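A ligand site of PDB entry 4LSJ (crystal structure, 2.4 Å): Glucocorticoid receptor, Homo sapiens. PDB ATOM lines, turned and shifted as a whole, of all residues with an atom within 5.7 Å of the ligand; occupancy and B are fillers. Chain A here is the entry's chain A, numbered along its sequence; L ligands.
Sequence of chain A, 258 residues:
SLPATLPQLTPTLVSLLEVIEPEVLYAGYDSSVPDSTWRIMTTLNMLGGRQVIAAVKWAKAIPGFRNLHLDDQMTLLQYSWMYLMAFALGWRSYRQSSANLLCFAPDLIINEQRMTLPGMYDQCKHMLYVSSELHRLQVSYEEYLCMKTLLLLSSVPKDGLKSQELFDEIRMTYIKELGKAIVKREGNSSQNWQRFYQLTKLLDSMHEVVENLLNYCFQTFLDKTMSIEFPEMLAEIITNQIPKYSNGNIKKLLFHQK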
ATOM      1  N   MET A  41      22.403  -4.881  17.133  1.00  0.00           N
ATOM      2  CA  MET A  41      21.929  -4.657  18.507  1.00  0.00           C
ATOM      3  C   MET A  41      22.782  -5.468  19.483  1.00  0.00           C
ATOM      4  O   MET A  41      23.314  -4.897  20.444  1.00  0.00           O
ATOM      5  CB  MET A  41      20.440  -5.036  18.706  1.00  0.00           C
ATOM      6  CG  MET A  41      19.550  -4.692  17.547  1.00  0.00           C
ATOM      7  SD  MET A  41      18.396  -3.348  17.878  1.00  0.00           S
ATOM      8  CE  MET A  41      17.075  -4.226  18.647  1.00  0.00           C
ATOM      9  N   LEU A  44      26.333  -4.174  19.677  1.00  0.00           N
ATOM     10  CA  LEU A  44      26.329  -2.905  20.396  1.00  0.00           C
ATOM     11  C   LEU A  44      26.209  -3.086  21.904  1.00  0.00           C
ATOM     12  O   LEU A  44      26.946  -2.429  22.652  1.00  0.00           O
ATOM     13  CB  LEU A  44      25.328  -1.900  19.828  1.00  0.00           C
ATOM     14  CG  LEU A  44      25.741  -1.327  18.454  1.00  0.00           C
ATOM     15  CD1 LEU A  44      24.649  -0.437  17.834  1.00  0.00           C
ATOM     16  CD2 LEU A  44      27.093  -0.625  18.522  1.00  0.00           C
ATOM     17  N   ASN A  45      25.359  -4.050  22.331  1.00  0.00           N
ATOM     18  CA  ASN A  45      25.186  -4.399  23.741  1.00  0.00           C
ATOM     19  C   ASN A  45      26.460  -5.010  24.270  1.00  0.00           C
ATOM     20  O   ASN A  45      26.826  -4.717  25.411  1.00  0.00           O
ATOM     21  CB  ASN A  45      24.033  -5.387  23.932  1.00  0.00           C
ATOM     22  CG  ASN A  45      22.675  -4.755  23.742  1.00  0.00           C
ATOM     23  OD1 ASN A  45      22.514  -3.534  23.669  1.00  0.00           O
ATOM     24  ND2 ASN A  45      21.656  -5.582  23.694  1.00  0.00           N
ATOM     25  N   LEU A  47      29.690  -4.595  23.058  1.00  0.00           N
ATOM     26  CA  LEU A  47      30.659  -3.499  23.147  1.00  0.00           C
ATOM     27  C   LEU A  47      30.299  -2.593  24.337  1.00  0.00           C
ATOM     28  O   LEU A  47      31.177  -2.247  25.141  1.00  0.00           O
ATOM     29  CB  LEU A  47      30.713  -2.720  21.817  1.00  0.00           C
ATOM     30  CG  LEU A  47      31.614  -1.487  21.734  1.00  0.00           C
ATOM     31  CD1 LEU A  47      33.130  -1.871  21.850  1.00  0.00           C
ATOM     32  CD2 LEU A  47      31.362  -0.741  20.472  1.00  0.00           C
ATOM     33  N   GLY A  48      28.993  -2.303  24.478  1.00  0.00           N
ATOM     34  CA  GLY A  48      28.431  -1.511  25.575  1.00  0.00           C
ATOM     35  C   GLY A  48      28.796  -2.056  26.941  1.00  0.00           C
ATOM     36  O   GLY A  48      29.222  -1.315  27.817  1.00  0.00           O
ATOM     37  N   GLY A  49      28.661  -3.369  27.116  1.00  0.00           N
ATOM     38  CA  GLY A  49      29.012  -4.048  28.364  1.00  0.00           C
ATOM     39  C   GLY A  49      30.495  -3.886  28.676  1.00  0.00           C
ATOM     40  O   GLY A  49      30.870  -3.530  29.796  1.00  0.00           O
ATOM     41  N   GLN A  51      32.419  -1.494  27.531  1.00  0.00           N
ATOM     42  CA  GLN A  51      32.594  -0.105  27.891  1.00  0.00           C
ATOM     43  C   GLN A  51      32.280   0.254  29.340  1.00  0.00           C
ATOM     44  O   GLN A  51      32.931   1.088  29.863  1.00  0.00           O
ATOM     45  CB  GLN A  51      31.823   0.840  26.981  1.00  0.00           C
ATOM     46  CG  GLN A  51      31.946   0.596  25.553  1.00  0.00           C
ATOM     47  CD  GLN A  51      32.648   1.662  24.852  1.00  0.00           C
ATOM     48  OE1 GLN A  51      32.446   1.866  23.701  1.00  0.00           O
ATOM     49  NE2 GLN A  51      33.484   2.357  25.531  1.00  0.00           N
ATOM     50  N   TRP A  81      26.584   5.390  33.834  1.00  0.00           N
ATOM     51  CA  TRP A  81      27.159   4.592  32.753  1.00  0.00           C
ATOM     52  C   TRP A  81      26.731   5.008  31.367  1.00  0.00           C
ATOM     53  O   TRP A  81      27.584   5.050  30.481  1.00  0.00           O
ATOM     54  CB  TRP A  81      27.015   3.067  32.972  1.00  0.00           C
ATOM     55  CG  TRP A  81      25.598   2.594  32.935  1.00  0.00           C
ATOM     56  CD1 TRP A  81      24.702   2.642  33.965  1.00  0.00           C
ATOM     57  CD2 TRP A  81      24.864   2.155  31.781  1.00  0.00           C
ATOM     58  NE1 TRP A  81      23.458   2.251  33.516  1.00  0.00           N
ATOM     59  CE2 TRP A  81      23.530   1.910  32.192  1.00  0.00           C
ATOM     60  CE3 TRP A  81      25.210   1.929  30.434  1.00  0.00           C
ATOM     61  CZ2 TRP A  81      22.565   1.398  31.331  1.00  0.00           C
ATOM     62  CZ3 TRP A  81      24.227   1.473  29.560  1.00  0.00           C
ATOM     63  CH2 TRP A  81      22.929   1.187  30.011  1.00  0.00           C
ATOM     64  N   MET A  82      25.447   5.386  31.183  1.00  0.00           N
ATOM     65  CA  MET A  82      24.956   5.800  29.868  1.00  0.00           C
ATOM     66  C   MET A  82      25.439   7.187  29.489  1.00  0.00           C
ATOM     67  O   MET A  82      25.573   7.479  28.297  1.00  0.00           O
ATOM     68  CB  MET A  82      23.426   5.651  29.727  1.00  0.00           C
ATOM     69  CG  MET A  82      22.909   5.785  28.278  1.00  0.00           C
ATOM     70  SD  MET A  82      23.477   4.491  27.120  1.00  0.00           S
ATOM     71  CE  MET A  82      22.139   3.415  27.215  1.00  0.00           C
ATOM     72  N   MET A  85      29.158   6.688  28.239  1.00  0.00           N
ATOM     73  CA  MET A  85      29.139   6.008  26.954  1.00  0.00           C
ATOM     74  C   MET A  85      28.666   6.879  25.826  1.00  0.00           C
ATOM     75  O   MET A  85      29.300   6.833  24.780  1.00  0.00           O
ATOM     76  CB  MET A  85      28.256   4.774  27.020  1.00  0.00           C
ATOM     77  CG  MET A  85      28.720   3.676  26.102  1.00  0.00           C
ATOM     78  SD  MET A  85      27.735   2.179  26.288  1.00  0.00           S
ATOM     79  CE  MET A  85      28.036   1.797  28.006  1.00  0.00           C
ATOM     80  N   ALA A  86      27.550   7.635  26.020  1.00  0.00           N
ATOM     81  CA  ALA A  86      26.987   8.524  24.993  1.00  0.00           C
ATOM     82  C   ALA A  86      27.911   9.693  24.691  1.00  0.00           C
ATOM     83  O   ALA A  86      28.101  10.038  23.527  1.00  0.00           O
ATOM     84  CB  ALA A  86      25.619   9.049  25.426  1.00  0.00           C
ATOM     85  N   LEU A  89      30.988   8.509  22.736  1.00  0.00           N
ATOM     86  CA  LEU A  89      30.507   8.201  21.388  1.00  0.00           C
ATOM     87  C   LEU A  89      30.382   9.498  20.568  1.00  0.00           C
ATOM     88  O   LEU A  89      30.803   9.529  19.402  1.00  0.00           O
ATOM     89  CB  LEU A  89      29.151   7.459  21.455  1.00  0.00           C
ATOM     90  CG  LEU A  89      28.423   7.192  20.100  1.00  0.00           C
ATOM     91  CD1 LEU A  89      29.222   6.237  19.215  1.00  0.00           C
ATOM     92  CD2 LEU A  89      27.007   6.690  20.312  1.00  0.00           C
ATOM     93  N   ARG A  92      34.112  10.600  19.852  1.00  0.00           N
ATOM     94  CA  ARG A  92      34.748   9.823  18.765  1.00  0.00           C
ATOM     95  C   ARG A  92      34.110  10.122  17.414  1.00  0.00           C
ATOM     96  O   ARG A  92      34.823  10.154  16.423  1.00  0.00           O
ATOM     97  CB  ARG A  92      34.695   8.320  19.032  1.00  0.00           C
ATOM     98  CG  ARG A  92      35.415   7.845  20.296  1.00  0.00           C
ATOM     99  CD  ARG A  92      35.467   6.315  20.373  1.00  0.00           C
ATOM    100  NE  ARG A  92      34.124   5.710  20.371  1.00  0.00           N
ATOM    101  CZ  ARG A  92      33.425   5.449  21.471  1.00  0.00           C
ATOM    102  NH1 ARG A  92      33.915   5.734  22.668  1.00  0.00           N
ATOM    103  NH2 ARG A  92      32.215   4.906  21.380  1.00  0.00           N
ATOM    104  N   LEU A 102      28.403   7.561  13.120  1.00  0.00           N
ATOM    105  CA  LEU A 102      28.529   7.342  14.553  1.00  0.00           C
ATOM    106  C   LEU A 102      29.597   6.326  14.787  1.00  0.00           C
ATOM    107  O   LEU A 102      29.453   5.151  14.409  1.00  0.00           O
ATOM    108  CB  LEU A 102      27.208   6.940  15.192  1.00  0.00           C
ATOM    109  CG  LEU A 102      26.258   8.078  15.494  1.00  0.00           C
ATOM    110  CD1 LEU A 102      25.031   7.557  16.088  1.00  0.00           C
ATOM    111  CD2 LEU A 102      26.862   9.096  16.448  1.00  0.00           C
ATOM    112  N   PHE A 104      30.995   4.114  17.008  1.00  0.00           N
ATOM    113  CA  PHE A 104      30.821   3.234  18.169  1.00  0.00           C
ATOM    114  C   PHE A 104      32.179   2.624  18.539  1.00  0.00           C
ATOM    115  O   PHE A 104      32.539   2.575  19.724  1.00  0.00           O
ATOM    116  CB  PHE A 104      29.742   2.171  17.907  1.00  0.00           C
ATOM    117  CG  PHE A 104      28.324   2.692  17.863  1.00  0.00           C
ATOM    118  CD1 PHE A 104      27.685   2.915  16.655  1.00  0.00           C
ATOM    119  CD2 PHE A 104      27.635   2.972  19.032  1.00  0.00           C
ATOM    120  CE1 PHE A 104      26.383   3.438  16.619  1.00  0.00           C
ATOM    121  CE2 PHE A 104      26.335   3.482  18.995  1.00  0.00           C
ATOM    122  CZ  PHE A 104      25.712   3.708  17.792  1.00  0.00           C
ATOM    123  N   MET A 120      16.478   2.550  16.611  1.00  0.00           N
ATOM    124  CA  MET A 120      17.912   2.733  16.470  1.00  0.00           C
ATOM    125  C   MET A 120      18.186   4.007  15.676  1.00  0.00           C
ATOM    126  O   MET A 120      19.147   4.734  15.966  1.00  0.00           O
ATOM    127  CB  MET A 120      18.514   1.499  15.785  1.00  0.00           C
ATOM    128  CG  MET A 120      19.955   1.645  15.367  1.00  0.00           C
ATOM    129  SD  MET A 120      21.098   1.740  16.748  1.00  0.00           S
ATOM    130  CE  MET A 120      22.649   1.778  15.864  1.00  0.00           C
ATOM    131  N   GLN A 123      17.688   6.966  18.097  1.00  0.00           N
ATOM    132  CA  GLN A 123      18.784   7.085  19.064  1.00  0.00           C
ATOM    133  C   GLN A 123      20.011   7.723  18.466  1.00  0.00           C
ATOM    134  O   GLN A 123      20.625   8.589  19.075  1.00  0.00           O
ATOM    135  CB  GLN A 123      19.123   5.733  19.704  1.00  0.00           C
ATOM    136  CG  GLN A 123      18.182   5.283  20.844  1.00  0.00           C
ATOM    137  CD  GLN A 123      17.073   6.231  21.213  1.00  0.00           C
ATOM    138  OE1 GLN A 123      17.287   7.257  21.865  1.00  0.00           O
ATOM    139  NE2 GLN A 123      15.866   5.894  20.810  1.00  0.00           N
ATOM    140  N   CYS A 124      20.347   7.274  17.256  1.00  0.00           N
ATOM    141  CA  CYS A 124      21.436   7.760  16.461  1.00  0.00           C
ATOM    142  C   CYS A 124      21.318   9.240  16.129  1.00  0.00           C
ATOM    143  O   CYS A 124      22.325   9.937  16.205  1.00  0.00           O
ATOM    144  CB  CYS A 124      21.601   6.905  15.216  1.00  0.00           C
ATOM    145  SG  CYS A 124      22.217   5.248  15.568  1.00  0.00           S
ATOM    146  N   MET A 127      22.296  11.294  19.097  1.00  0.00           N
ATOM    147  CA  MET A 127      23.739  11.200  19.220  1.00  0.00           C
ATOM    148  C   MET A 127      24.411  12.146  18.249  1.00  0.00           C
ATOM    149  O   MET A 127      25.444  12.740  18.562  1.00  0.00           O
ATOM    150  CB  MET A 127      24.228   9.757  18.964  1.00  0.00           C
ATOM    151  CG  MET A 127      23.914   8.792  20.088  1.00  0.00           C
ATOM    152  SD  MET A 127      24.363   9.413  21.745  1.00  0.00           S
ATOM    153  CE  MET A 127      26.052  10.023  21.447  1.00  0.00           C
ATOM    154  N   LEU A 213      18.035   7.369  25.441  1.00  0.00           N
ATOM    155  CA  LEU A 213      18.855   6.159  25.257  1.00  0.00           C
ATOM    156  C   LEU A 213      18.477   5.068  26.279  1.00  0.00           C
ATOM    157  O   LEU A 213      18.335   3.901  25.890  1.00  0.00           O
ATOM    158  CB  LEU A 213      20.357   6.483  25.353  1.00  0.00           C
ATOM    159  CG  LEU A 213      20.939   7.338  24.248  1.00  0.00           C
ATOM    160  CD1 LEU A 213      22.332   7.781  24.603  1.00  0.00           C
ATOM    161  CD2 LEU A 213      20.958   6.593  22.906  1.00  0.00           C
ATOM    162  N   LEU A 214      18.321   5.444  27.578  1.00  0.00           N
ATOM    163  CA  LEU A 214      17.944   4.496  28.628  1.00  0.00           C
ATOM    164  C   LEU A 214      16.562   3.906  28.366  1.00  0.00           C
ATOM    165  O   LEU A 214      16.376   2.708  28.574  1.00  0.00           O
ATOM    166  CB  LEU A 214      17.955   5.147  30.018  1.00  0.00           C
ATOM    167  CG  LEU A 214      19.320   5.405  30.643  1.00  0.00           C
ATOM    168  CD1 LEU A 214      19.174   6.107  31.978  1.00  0.00           C
ATOM    169  CD2 LEU A 214      20.155   4.107  30.783  1.00  0.00           C
ATOM    170  N   TYR A 216      15.046   3.384  25.370  1.00  0.00           N
ATOM    171  CA  TYR A 216      15.147   2.422  24.285  1.00  0.00           C
ATOM    172  C   TYR A 216      15.796   1.149  24.784  1.00  0.00           C
ATOM    173  O   TYR A 216      15.348   0.054  24.449  1.00  0.00           O
ATOM    174  CB  TYR A 216      15.941   3.026  23.113  1.00  0.00           C
ATOM    175  CG  TYR A 216      16.155   2.102  21.923  1.00  0.00           C
ATOM    176  CD1 TYR A 216      17.436   1.792  21.486  1.00  0.00           C
ATOM    177  CD2 TYR A 216      15.073   1.574  21.221  1.00  0.00           C
ATOM    178  CE1 TYR A 216      17.632   0.980  20.360  1.00  0.00           C
ATOM    179  CE2 TYR A 216      15.261   0.744  20.107  1.00  0.00           C
ATOM    180  CZ  TYR A 216      16.544   0.469  19.681  1.00  0.00           C
ATOM    181  OH  TYR A 216      16.754  -0.368  18.612  1.00  0.00           O
ATOM    182  N   CYS A 217      16.831   1.301  25.615  1.00  0.00           N
ATOM    183  CA  CYS A 217      17.586   0.226  26.241  1.00  0.00           C
ATOM    184  C   CYS A 217      16.693  -0.608  27.147  1.00  0.00           C
ATOM    185  O   CYS A 217      16.698  -1.828  27.046  1.00  0.00           O
ATOM    186  CB  CYS A 217      18.769   0.807  27.000  1.00  0.00           C
ATOM    187  SG  CYS A 217      19.901  -0.433  27.630  1.00  0.00           S
ATOM    188  N   THR A 220      14.091  -2.632  24.973  1.00  0.00           N
ATOM    189  CA  THR A 220      14.717  -3.809  24.399  1.00  0.00           C
ATOM    190  C   THR A 220      15.028  -4.861  25.460  1.00  0.00           C
ATOM    191  O   THR A 220      14.698  -6.024  25.242  1.00  0.00           O
ATOM    192  CB  THR A 220      15.932  -3.450  23.559  1.00  0.00           C
ATOM    193  OG1 THR A 220      15.677  -2.239  22.846  1.00  0.00           O
ATOM    194  CG2 THR A 220      16.301  -4.547  22.575  1.00  0.00           C
ATOM    195  N   PHE A 221      15.610  -4.461  26.605  1.00  0.00           N
ATOM    196  CA  PHE A 221      15.963  -5.370  27.703  1.00  0.00           C
ATOM    197  C   PHE A 221      14.781  -6.211  28.193  1.00  0.00           C
ATOM    198  O   PHE A 221      14.957  -7.373  28.536  1.00  0.00           O
ATOM    199  CB  PHE A 221      16.577  -4.611  28.890  1.00  0.00           C
ATOM    200  CG  PHE A 221      17.091  -5.507  30.005  1.00  0.00           C
ATOM    201  CD1 PHE A 221      18.268  -6.238  29.836  1.00  0.00           C
ATOM    202  CD2 PHE A 221      16.379  -5.656  31.188  1.00  0.00           C
ATOM    203  CE1 PHE A 221      18.728  -7.090  30.853  1.00  0.00           C
ATOM    204  CE2 PHE A 221      16.846  -6.478  32.205  1.00  0.00           C
ATOM    205  CZ  PHE A 221      18.025  -7.187  32.037  1.00  0.00           C
ATOM    206  N   ILE A 228      17.092  -9.897  22.242  1.00  0.00           N
ATOM    207  CA  ILE A 228      18.387  -9.375  21.889  1.00  0.00           C
ATOM    208  C   ILE A 228      19.257  -9.710  23.117  1.00  0.00           C
ATOM    209  O   ILE A 228      18.793  -9.579  24.253  1.00  0.00           O
ATOM    210  CB  ILE A 228      18.289  -7.827  21.639  1.00  0.00           C
ATOM    211  CG1 ILE A 228      17.365  -7.457  20.439  1.00  0.00           C
ATOM    212  CG2 ILE A 228      19.663  -7.132  21.564  1.00  0.00           C
ATOM    213  CD1 ILE A 228      17.790  -7.953  18.991  1.00  0.00           C
ATOM    214  N   PHE A 230      22.246  -9.429  25.937  1.00  0.00           N
ATOM    215  CA  PHE A 230      22.894  -8.429  26.762  1.00  0.00           C
ATOM    216  C   PHE A 230      23.983  -9.130  27.571  1.00  0.00           C
ATOM    217  O   PHE A 230      23.726 -10.214  28.088  1.00  0.00           O
ATOM    218  CB  PHE A 230      21.894  -7.777  27.730  1.00  0.00           C
ATOM    219  CG  PHE A 230      21.006  -6.727  27.121  1.00  0.00           C
ATOM    220  CD1 PHE A 230      19.904  -7.076  26.351  1.00  0.00           C
ATOM    221  CD2 PHE A 230      21.205  -5.374  27.399  1.00  0.00           C
ATOM    222  CE1 PHE A 230      19.054  -6.099  25.811  1.00  0.00           C
ATOM    223  CE2 PHE A 230      20.361  -4.410  26.866  1.00  0.00           C
ATOM    224  CZ  PHE A 230      19.283  -4.775  26.088  1.00  0.00           C
ATOM    225  N   LEU A 234      26.040  -5.543  32.091  1.00  0.00           N
ATOM    226  CA  LEU A 234      25.081  -4.566  31.593  1.00  0.00           C
ATOM    227  C   LEU A 234      23.702  -4.982  32.123  1.00  0.00           C
ATOM    228  O   LEU A 234      22.971  -4.154  32.677  1.00  0.00           O
ATOM    229  CB  LEU A 234      25.069  -4.557  30.052  1.00  0.00           C
ATOM    230  CG  LEU A 234      24.077  -3.642  29.352  1.00  0.00           C
ATOM    231  CD1 LEU A 234      24.387  -2.197  29.675  1.00  0.00           C
ATOM    232  CD2 LEU A 234      24.085  -3.828  27.835  1.00  0.00           C
HETATM  233  C1  LIG L   1      25.432   4.599  23.458  1.00  0.00           C
HETATM  234  O1  LIG L   1      26.787   4.477  23.104  1.00  0.00           O
HETATM  235  C2  LIG L   1      27.262   3.206  22.851  1.00  0.00           C
HETATM  236  C3  LIG L   1      26.529   2.044  22.784  1.00  0.00           C
HETATM  237  C4  LIG L   1      27.161   0.875  22.512  1.00  0.00           C
HETATM  238  C5  LIG L   1      28.509   0.790  22.328  1.00  0.00           C
HETATM  239  C6  LIG L   1      29.243   1.929  22.405  1.00  0.00           C
HETATM  240  C7  LIG L   1      28.613   3.107  22.667  1.00  0.00           C
HETATM  241  C8  LIG L   1      25.113   2.034  22.909  1.00  0.00           C
HETATM  242  C9  LIG L   1      24.454   1.229  23.758  1.00  0.00           C
HETATM  243  C10 LIG L   1      23.015   1.178  23.815  1.00  0.00           C
HETATM  244  C11 LIG L   1      22.155   2.222  23.970  1.00  0.00           C
HETATM  245  C12 LIG L   1      20.797   2.039  24.005  1.00  0.00           C
HETATM  246  C13 LIG L   1      20.228   0.796  23.885  1.00  0.00           C
HETATM  247  C14 LIG L   1      21.096  -0.254  23.727  1.00  0.00           C
HETATM  248  C15 LIG L   1      22.443  -0.051  23.696  1.00  0.00           C
HETATM  249  N1  LIG L   1      20.736  -1.597  23.612  1.00  0.00           N
HETATM  250  S1  LIG L   1      19.450  -2.187  22.748  1.00  0.00           S
HETATM  251  O2  LIG L   1      19.402  -3.570  22.873  1.00  0.00           O
HETATM  252  O3  LIG L   1      18.277  -1.473  22.998  1.00  0.00           O
HETATM  253  C16 LIG L   1      20.016  -1.825  21.160  1.00  0.00           C
HETATM  254  C17 LIG L   1      25.113   0.267  24.659  1.00  0.00           C
HETATM  255  C18 LIG L   1      24.537   0.248  26.039  1.00  0.00           C
HETATM  256  C19 LIG L   1      24.366   2.912  22.051  1.00  0.00           C
HETATM  257  C20 LIG L   1      24.529   4.241  22.338  1.00  0.00           C
HETATM  258  C21 LIG L   1      23.841   5.157  21.589  1.00  0.00           C
HETATM  259  C22 LIG L   1      23.020   4.762  20.567  1.00  0.00           C
HETATM  260  C23 LIG L   1      22.874   3.436  20.286  1.00  0.00           C
HETATM  261  C24 LIG L   1      23.548   2.504  21.027  1.00  0.00           C
HETATM  262  O4  LIG L   1      23.431   1.184  20.748  1.00  0.00           O
HETATM  263  C25 LIG L   1      22.260   0.955  20.057  1.00  0.00           C
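OD1 of Asn 45 is in hydrogen-bond range of N1 of the ligand (2.6 Å). The side-chain hydroxyl (OG1) of Thr 220 lies within hydrogen-bond range of an oxygen (O3) of the ligand, 2.7 Å away.
OG1 of Thr 220 lies within hydrogen-bond range of O of Tyr 216 (2.8 Å). O of Phe 104 is in hydrogen-bond range of NH2 of Arg 92, 2.9 Å away. SG of Cys 124 sits at hydrogen-bond distance from O of Met 120 (3.1 Å). The side-chain hydroxyl (OH) of Tyr 216 sits at hydrogen-bond distance from the side-chain sulfur (SD) of Met 41 (3.5 Å).
Met 41 touches the ligand. Leu 44 touches the ligand. CD2 of Leu 47 touches C5 of the ligand (3.7 Å). N of Gly 48 touches C5 of the ligand, at 3.8 Å. Gln 51 touches the ligand (OE1 to C6, 3.5 Å). CZ3 of Trp 81 touches C18 of the ligand (3.7 Å). Met 82 touches the ligand. CG of Met 85 touches C7 of the ligand (3.5 Å). CD2 of Leu 89 touches O1 of the ligand, 3.6 Å away. Phe 104 touches the ligand (CE2 to C24, 3.6 Å). Met 120 touches the ligand. Met 127 touches the ligand (CG to C21, 3.9 Å). CD2 of Leu 213 touches C21 of the ligand, 3.5 Å away. Tyr 216 touches the ligand (O to O3, 3.6 Å). CB of Cys 217 touches C13 of the ligand (3.4 Å). Ile 228 touches the ligand. Phe 230 touches the ligand (CZ to O2, 3.4 Å). Hydrophobic or aromatic side chains within 4 Å of the ligand: Met 41, Leu 44, Leu 47, Trp 81, Met 82, Met 85, Leu 89, Phe 104, Met 120, Met 127, Leu 213, Tyr 216, Ile 228 and Phe 230. 19 residues have an atom within 4 Å of the ligand: Met 41, Leu 44, Asn 45, Leu 47, Gly 48, Gln 51, Trp 81, Met 82, Met 85, Leu 89, Phe 104, Met 120, Met 127, Leu 213, Tyr 216, Cys 217, Thr 220, Ile 228 and Phe 230. The nearest printed residue that does not touch the ligand is Gln 123 (4.1 Å).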
